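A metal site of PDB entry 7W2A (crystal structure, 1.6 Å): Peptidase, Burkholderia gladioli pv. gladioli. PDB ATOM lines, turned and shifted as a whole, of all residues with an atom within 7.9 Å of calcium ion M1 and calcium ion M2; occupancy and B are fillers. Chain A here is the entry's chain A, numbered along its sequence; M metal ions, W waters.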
ATOM      1  N   TYR A  59      -4.086  -7.283 -19.250  1.00  0.00           N
ATOM      2  CA  TYR A  59      -4.865  -6.504 -20.186  1.00  0.00           C
ATOM      3  C   TYR A  59      -5.558  -7.427 -21.158  1.00  0.00           C
ATOM      4  O   TYR A  59      -5.116  -8.561 -21.402  1.00  0.00           O
ATOM      5  CB  TYR A  59      -4.014  -5.482 -20.950  1.00  0.00           C
ATOM      6  CG  TYR A  59      -4.770  -4.226 -21.298  1.00  0.00           C
ATOM      7  CD1 TYR A  59      -4.953  -3.244 -20.339  1.00  0.00           C
ATOM      8  CD2 TYR A  59      -5.288  -4.014 -22.577  1.00  0.00           C
ATOM      9  CE1 TYR A  59      -5.650  -2.082 -20.630  1.00  0.00           C
ATOM     10  CE2 TYR A  59      -5.980  -2.856 -22.881  1.00  0.00           C
ATOM     11  CZ  TYR A  59      -6.150  -1.906 -21.899  1.00  0.00           C
ATOM     12  OH  TYR A  59      -6.826  -0.730 -22.197  1.00  0.00           O
ATOM     13  N   ASP A  60      -6.656  -6.928 -21.723  1.00  0.00           N
ATOM     14  CA  ASP A  60      -7.515  -7.681 -22.632  1.00  0.00           C
ATOM     15  C   ASP A  60      -7.534  -6.930 -23.954  1.00  0.00           C
ATOM     16  O   ASP A  60      -8.154  -5.861 -24.059  1.00  0.00           O
ATOM     17  CB  ASP A  60      -8.917  -7.837 -22.027  1.00  0.00           C
ATOM     18  CG  ASP A  60      -9.817  -8.750 -22.837  1.00  0.00           C
ATOM     19  OD1 ASP A  60      -9.609  -8.933 -24.063  1.00  0.00           O
ATOM     20  OD2 ASP A  60     -10.795  -9.243 -22.220  1.00  0.00           O
ATOM     21  N   PHE A  61      -6.832  -7.475 -24.950  1.00  0.00           N
ATOM     22  CA  PHE A  61      -6.702  -6.816 -26.241  1.00  0.00           C
ATOM     23  C   PHE A  61      -7.718  -7.287 -27.283  1.00  0.00           C
ATOM     24  O   PHE A  61      -7.600  -6.927 -28.452  1.00  0.00           O
ATOM     25  CB  PHE A  61      -5.275  -6.998 -26.763  1.00  0.00           C
ATOM     26  CG  PHE A  61      -4.296  -6.088 -26.097  1.00  0.00           C
ATOM     27  CD1 PHE A  61      -4.203  -4.755 -26.493  1.00  0.00           C
ATOM     28  CD2 PHE A  61      -3.526  -6.530 -25.036  1.00  0.00           C
ATOM     29  CE1 PHE A  61      -3.352  -3.901 -25.851  1.00  0.00           C
ATOM     30  CE2 PHE A  61      -2.660  -5.658 -24.387  1.00  0.00           C
ATOM     31  CZ  PHE A  61      -2.578  -4.348 -24.803  1.00  0.00           C
ATOM     32  N   ILE A  62      -8.720  -8.074 -26.884  1.00  0.00           N
ATOM     33  CA  ILE A  62      -9.707  -8.506 -27.874  1.00  0.00           C
ATOM     34  C   ILE A  62     -10.575  -7.318 -28.261  1.00  0.00           C
ATOM     35  O   ILE A  62     -11.305  -6.768 -27.431  1.00  0.00           O
ATOM     36  CB  ILE A  62     -10.555  -9.668 -27.352  1.00  0.00           C
ATOM     37  CG1 ILE A  62      -9.666 -10.865 -26.971  1.00  0.00           C
ATOM     38  CG2 ILE A  62     -11.535 -10.097 -28.450  1.00  0.00           C
ATOM     39  CD1 ILE A  62     -10.478 -12.029 -26.368  1.00  0.00           C
ATOM     40  N   SER A  63     -10.490  -6.915 -29.525  1.00  0.00           N
ATOM     41  CA  SER A  63     -11.140  -5.681 -29.972  1.00  0.00           C
ATOM     42  C   SER A  63     -12.624  -5.846 -30.245  1.00  0.00           C
ATOM     43  O   SER A  63     -13.402  -4.900 -30.053  1.00  0.00           O
ATOM     44  CB  SER A  63     -10.444  -5.168 -31.232  1.00  0.00           C
ATOM     45  OG  SER A  63      -9.095  -4.840 -30.961  1.00  0.00           O
ATOM     46  N   ASP A  64     -13.037  -7.037 -30.691  1.00  0.00           N
ATOM     47  CA  ASP A  64     -14.416  -7.277 -31.109  1.00  0.00           C
ATOM     48  C   ASP A  64     -15.232  -7.737 -29.912  1.00  0.00           C
ATOM     49  O   ASP A  64     -14.922  -8.802 -29.343  1.00  0.00           O
ATOM     50  CB  ASP A  64     -14.445  -8.322 -32.220  1.00  0.00           C
ATOM     51  CG  ASP A  64     -15.824  -8.507 -32.833  1.00  0.00           C
ATOM     52  OD1 ASP A  64     -16.831  -7.973 -32.323  1.00  0.00           O
ATOM     53  OD2 ASP A  64     -15.906  -9.192 -33.873  1.00  0.00           O
ATOM     54  N   PRO A  65     -16.271  -7.008 -29.505  1.00  0.00           N
ATOM     55  CA  PRO A  65     -17.042  -7.453 -28.329  1.00  0.00           C
ATOM     56  C   PRO A  65     -17.687  -8.813 -28.487  1.00  0.00           C
ATOM     57  O   PRO A  65     -17.851  -9.506 -27.477  1.00  0.00           O
ATOM     58  CB  PRO A  65     -18.094  -6.347 -28.161  1.00  0.00           C
ATOM     59  CG  PRO A  65     -17.479  -5.135 -28.821  1.00  0.00           C
ATOM     60  CD  PRO A  65     -16.687  -5.679 -29.982  1.00  0.00           C
ATOM     61  N   SER A  67     -16.490 -11.593 -30.063  1.00  0.00           N
ATOM     62  CA  SER A  67     -15.460 -12.563 -29.683  1.00  0.00           C
ATOM     63  C   SER A  67     -15.043 -12.401 -28.237  1.00  0.00           C
ATOM     64  O   SER A  67     -14.795 -13.395 -27.532  1.00  0.00           O
ATOM     65  CB  SER A  67     -14.234 -12.398 -30.589  1.00  0.00           C
ATOM     66  OG  SER A  67     -13.223 -13.301 -30.198  1.00  0.00           O
ATOM     67  N   ALA A  68     -14.947 -11.159 -27.756  1.00  0.00           N
ATOM     68  CA  ALA A  68     -14.469 -10.917 -26.401  1.00  0.00           C
ATOM     69  C   ALA A  68     -15.403 -11.514 -25.355  1.00  0.00           C
ATOM     70  O   ALA A  68     -14.947 -11.954 -24.298  1.00  0.00           O
ATOM     71  CB  ALA A  68     -14.322  -9.408 -26.174  1.00  0.00           C
ATOM     72  N   ASN A  69     -16.715 -11.520 -25.623  1.00  0.00           N
ATOM     73  CA  ASN A  69     -17.671 -12.242 -24.763  1.00  0.00           C
ATOM     74  C   ASN A  69     -17.688 -11.685 -23.343  1.00  0.00           C
ATOM     75  O   ASN A  69     -17.974 -12.410 -22.386  1.00  0.00           O
ATOM     76  CB  ASN A  69     -17.370 -13.744 -24.774  1.00  0.00           C
ATOM     77  CG  ASN A  69     -18.548 -14.580 -24.325  1.00  0.00           C
ATOM     78  OD1 ASN A  69     -19.696 -14.179 -24.464  1.00  0.00           O
ATOM     79  ND2 ASN A  69     -18.267 -15.765 -23.813  1.00  0.00           N
ATOM     80  N   ASP A  70     -17.382 -10.391 -23.175  1.00  0.00           N
ATOM     81  CA  ASP A  70     -17.292  -9.798 -21.847  1.00  0.00           C
ATOM     82  C   ASP A  70     -17.956  -8.421 -21.792  1.00  0.00           C
ATOM     83  O   ASP A  70     -17.774  -7.693 -20.795  1.00  0.00           O
ATOM     84  CB  ASP A  70     -15.826  -9.696 -21.389  1.00  0.00           C
ATOM     85  CG  ASP A  70     -15.007  -8.780 -22.254  1.00  0.00           C
ATOM     86  OD1 ASP A  70     -15.547  -8.249 -23.251  1.00  0.00           O
ATOM     87  OD2 ASP A  70     -13.801  -8.580 -21.958  1.00  0.00           O
ATOM     88  N   GLY A  71     -18.703  -8.046 -22.816  1.00  0.00           N
ATOM     89  CA  GLY A  71     -19.474  -6.822 -22.794  1.00  0.00           C
ATOM     90  C   GLY A  71     -18.794  -5.598 -23.383  1.00  0.00           C
ATOM     91  O   GLY A  71     -19.390  -4.510 -23.346  1.00  0.00           O
ATOM     92  N   ASN A  72     -17.582  -5.730 -23.913  1.00  0.00           N
ATOM     93  CA  ASN A  72     -16.914  -4.569 -24.485  1.00  0.00           C
ATOM     94  C   ASN A  72     -15.702  -5.025 -25.294  1.00  0.00           C
ATOM     95  O   ASN A  72     -15.302  -6.199 -25.275  1.00  0.00           O
ATOM     96  CB  ASN A  72     -16.495  -3.579 -23.384  1.00  0.00           C
ATOM     97  CG  ASN A  72     -15.787  -4.240 -22.243  1.00  0.00           C
ATOM     98  OD1 ASN A  72     -14.939  -5.095 -22.449  1.00  0.00           O
ATOM     99  ND2 ASN A  72     -16.128  -3.859 -21.015  1.00  0.00           N
ATOM    100  N   GLY A  73     -15.109  -4.063 -26.007  1.00  0.00           N
ATOM    101  CA  GLY A  73     -13.856  -4.288 -26.712  1.00  0.00           C
ATOM    102  C   GLY A  73     -12.666  -4.294 -25.759  1.00  0.00           C
ATOM    103  O   GLY A  73     -12.760  -4.831 -24.658  1.00  0.00           O
ATOM    104  N   ARG A  74     -11.561  -3.676 -26.148  1.00  0.00           N
ATOM    105  CA  ARG A  74     -10.354  -3.776 -25.331  1.00  0.00           C
ATOM    106  C   ARG A  74     -10.611  -3.224 -23.926  1.00  0.00           C
ATOM    107  O   ARG A  74     -11.380  -2.278 -23.739  1.00  0.00           O
ATOM    108  CB  ARG A  74      -9.205  -3.047 -25.997  1.00  0.00           C
ATOM    109  CG  ARG A  74      -8.770  -3.737 -27.284  1.00  0.00           C
ATOM    110  CD  ARG A  74      -7.404  -3.223 -27.749  1.00  0.00           C
ATOM    111  NE  ARG A  74      -6.896  -4.048 -28.838  1.00  0.00           N
ATOM    112  CZ  ARG A  74      -5.856  -3.729 -29.598  1.00  0.00           C
ATOM    113  NH1 ARG A  74      -5.191  -2.594 -29.377  1.00  0.00           N
ATOM    114  NH2 ARG A  74      -5.476  -4.536 -30.586  1.00  0.00           N
ATOM    115  N   ASP A  75      -9.997  -3.856 -22.927  1.00  0.00           N
ATOM    116  CA  ASP A  75     -10.281  -3.496 -21.541  1.00  0.00           C
ATOM    117  C   ASP A  75      -9.145  -3.999 -20.651  1.00  0.00           C
ATOM    118  O   ASP A  75      -8.266  -4.753 -21.096  1.00  0.00           O
ATOM    119  CB  ASP A  75     -11.646  -4.064 -21.098  1.00  0.00           C
ATOM    120  CG  ASP A  75     -11.650  -5.584 -20.979  1.00  0.00           C
ATOM    121  OD1 ASP A  75     -11.189  -6.072 -19.935  1.00  0.00           O
ATOM    122  OD2 ASP A  75     -12.131  -6.280 -21.890  1.00  0.00           O
ATOM    123  N   ASN A  76      -9.158  -3.572 -19.391  1.00  0.00           N
ATOM    124  CA  ASN A  76      -8.054  -3.865 -18.485  1.00  0.00           C
ATOM    125  C   ASN A  76      -8.273  -5.110 -17.622  1.00  0.00           C
ATOM    126  O   ASN A  76      -7.539  -5.310 -16.649  1.00  0.00           O
ATOM    127  CB  ASN A  76      -7.755  -2.648 -17.595  1.00  0.00           C
ATOM    128  CG  ASN A  76      -8.851  -2.352 -16.597  1.00  0.00           C
ATOM    129  OD1 ASN A  76      -9.880  -3.028 -16.537  1.00  0.00           O
ATOM    130  ND2 ASN A  76      -8.621  -1.327 -15.779  1.00  0.00           N
ATOM    131  N   ASN A  77      -9.220  -5.969 -17.990  1.00  0.00           N
ATOM    132  CA  ASN A  77      -9.554  -7.165 -17.204  1.00  0.00           C
ATOM    133  C   ASN A  77      -9.329  -8.394 -18.088  1.00  0.00           C
ATOM    134  O   ASN A  77     -10.170  -8.719 -18.939  1.00  0.00           O
ATOM    135  CB  ASN A  77     -10.992  -7.100 -16.688  1.00  0.00           C
ATOM    136  CG  ASN A  77     -11.360  -8.294 -15.820  1.00  0.00           C
ATOM    137  OD1 ASN A  77     -10.568  -9.222 -15.648  1.00  0.00           O
ATOM    138  ND2 ASN A  77     -12.563  -8.270 -15.261  1.00  0.00           N
ATOM    139  N   ALA A  78      -8.213  -9.094 -17.842  1.00  0.00           N
ATOM    140  CA  ALA A  78      -7.837 -10.274 -18.621  1.00  0.00           C
ATOM    141  C   ALA A  78      -8.468 -11.562 -18.114  1.00  0.00           C
ATOM    142  O   ALA A  78      -8.058 -12.652 -18.529  1.00  0.00           O
ATOM    143  CB  ALA A  78      -6.302 -10.408 -18.656  1.00  0.00           C
ATOM    144  N   ALA A  79      -9.473 -11.484 -17.249  1.00  0.00           N
ATOM    145  CA  ALA A  79     -10.207 -12.694 -16.893  1.00  0.00           C
ATOM    146  C   ALA A  79     -10.873 -13.324 -18.120  1.00  0.00           C
ATOM    147  O   ALA A  79     -11.308 -12.636 -19.046  1.00  0.00           O
ATOM    148  CB  ALA A  79     -11.266 -12.373 -15.828  1.00  0.00           C
ATOM    149  N   ASP A  80     -10.927 -14.658 -18.114  1.00  0.00           N
ATOM    150  CA  ASP A  80     -11.488 -15.414 -19.227  1.00  0.00           C
ATOM    151  C   ASP A  80     -12.979 -15.629 -18.959  1.00  0.00           C
ATOM    152  O   ASP A  80     -13.331 -16.355 -18.016  1.00  0.00           O
ATOM    153  CB  ASP A  80     -10.771 -16.756 -19.369  1.00  0.00           C
ATOM    154  CG  ASP A  80     -11.149 -17.530 -20.626  1.00  0.00           C
ATOM    155  OD1 ASP A  80     -12.069 -17.122 -21.368  1.00  0.00           O
ATOM    156  OD2 ASP A  80     -10.520 -18.598 -20.883  1.00  0.00           O
ATOM    157  N   PRO A  81     -13.877 -15.035 -19.752  1.00  0.00           N
ATOM    158  CA  PRO A  81     -15.312 -15.292 -19.569  1.00  0.00           C
ATOM    159  C   PRO A  81     -15.758 -16.605 -20.158  1.00  0.00           C
ATOM    160  O   PRO A  81     -16.930 -16.978 -19.969  1.00  0.00           O
ATOM    161  CB  PRO A  81     -15.959 -14.122 -20.314  1.00  0.00           C
ATOM    162  CG  PRO A  81     -15.037 -13.942 -21.504  1.00  0.00           C
ATOM    163  CD  PRO A  81     -13.626 -14.110 -20.877  1.00  0.00           C
ATOM    164  N   ARG A 147      -4.933 -11.149 -22.541  1.00  0.00           N
ATOM    165  CA  ARG A 147      -6.018 -11.887 -23.179  1.00  0.00           C
ATOM    166  C   ARG A 147      -6.144 -11.426 -24.624  1.00  0.00           C
ATOM    167  O   ARG A 147      -6.375 -10.251 -24.891  1.00  0.00           O
ATOM    168  CB  ARG A 147      -7.323 -11.706 -22.407  1.00  0.00           C
ATOM    169  CG  ARG A 147      -8.530 -12.351 -23.092  1.00  0.00           C
ATOM    170  CD  ARG A 147      -9.715 -12.503 -22.152  1.00  0.00           C
ATOM    171  NE  ARG A 147     -10.735 -13.315 -22.824  1.00  0.00           N
ATOM    172  CZ  ARG A 147     -11.880 -12.828 -23.331  1.00  0.00           C
ATOM    173  NH1 ARG A 147     -12.193 -11.549 -23.176  1.00  0.00           N
ATOM    174  NH2 ARG A 147     -12.700 -13.646 -23.958  1.00  0.00           N
HETATM  175 CA    CA M   1     -12.039  -8.345 -20.402  1.00  0.00          CA
HETATM  176 CA    CA M   2     -13.660  -6.665 -23.531  1.00  0.00          CA
HETATM  177  O   HOH W   1     -13.716  -7.497 -18.914  1.00  0.00           O
HETATM  178  O   HOH W   2     -12.734 -10.411 -19.493  1.00  0.00           O
HETATM  179  O   HOH W   3     -11.976  -7.709 -24.878  1.00  0.00           O
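The side-chain carboxylate (OD2) of Asp 70 lies close to the guanidinium group (NH1) of Arg 147, at 3.6 Å.
The backbone NH (N) of Ile 62 is in hydrogen-bond range of the side-chain carboxylate (OD1) of Asp 60, 3.1 Å away.
The backbone carbonyl oxygen of Ala 68 sits at hydrogen-bond distance from the guanidinium group of Arg 147, at 2.8 Å.
OD1 of Asn 77 lies within hydrogen-bond range of N of Ala 79 (3.0 Å).
NH1 of Arg 147 is in salt-bridge range of OD1 of Asp 60 (3.8 Å).
Within 4 Å of calcium ion M1: Asp 60, Asp 70, Asp 75 and Asn 77.
The nearest printed residue that does not touch calcium ion M1 is Arg 147 (4.2 Å).
CB of Ala 68 touches calcium ion M2 (3.9 Å).
Of the 23 residues printed, 5 come within 4 Å of calcium ion M2.
Water W2 is bound to calcium ion M1.
OD2 of Asp 70 binds calcium ion M1 (2.4 Å).
OD2 of Asp 60 is bound to calcium ion M1 (2.4 Å).
Water W1 binds calcium ion M1 (2.4 Å).
Calcium ion M1 is bound by O of Asn 77 (2.4 Å).
The side-chain carboxylate (OD1) of Asp 75 binds calcium ion M1.
OD2 of Asp 75 binds calcium ion M1 (2.5 Å).
Calcium ion M1 has seven donor atoms within binding distance.
Calcium ion M2 is bound by the side-chain carboxylate (OD2) of Asp 75, the side-chain amide oxygen (OD1) of Asn 72, the backbone carbonyl oxygen (O) of Gly 73, water W3, the backbone carbonyl oxygen (O) of Asn 72, the side-chain carboxylate (OD1) of Asp 70 and the side-chain carboxylate (OD2) of Asp 70.
Water W3 lies within hydrogen-bond range of the side-chain carboxylate (OD1) of Asp 60 (2.8 Å) and the backbone carbonyl oxygen (O) of Ile 62 (2.8 Å).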
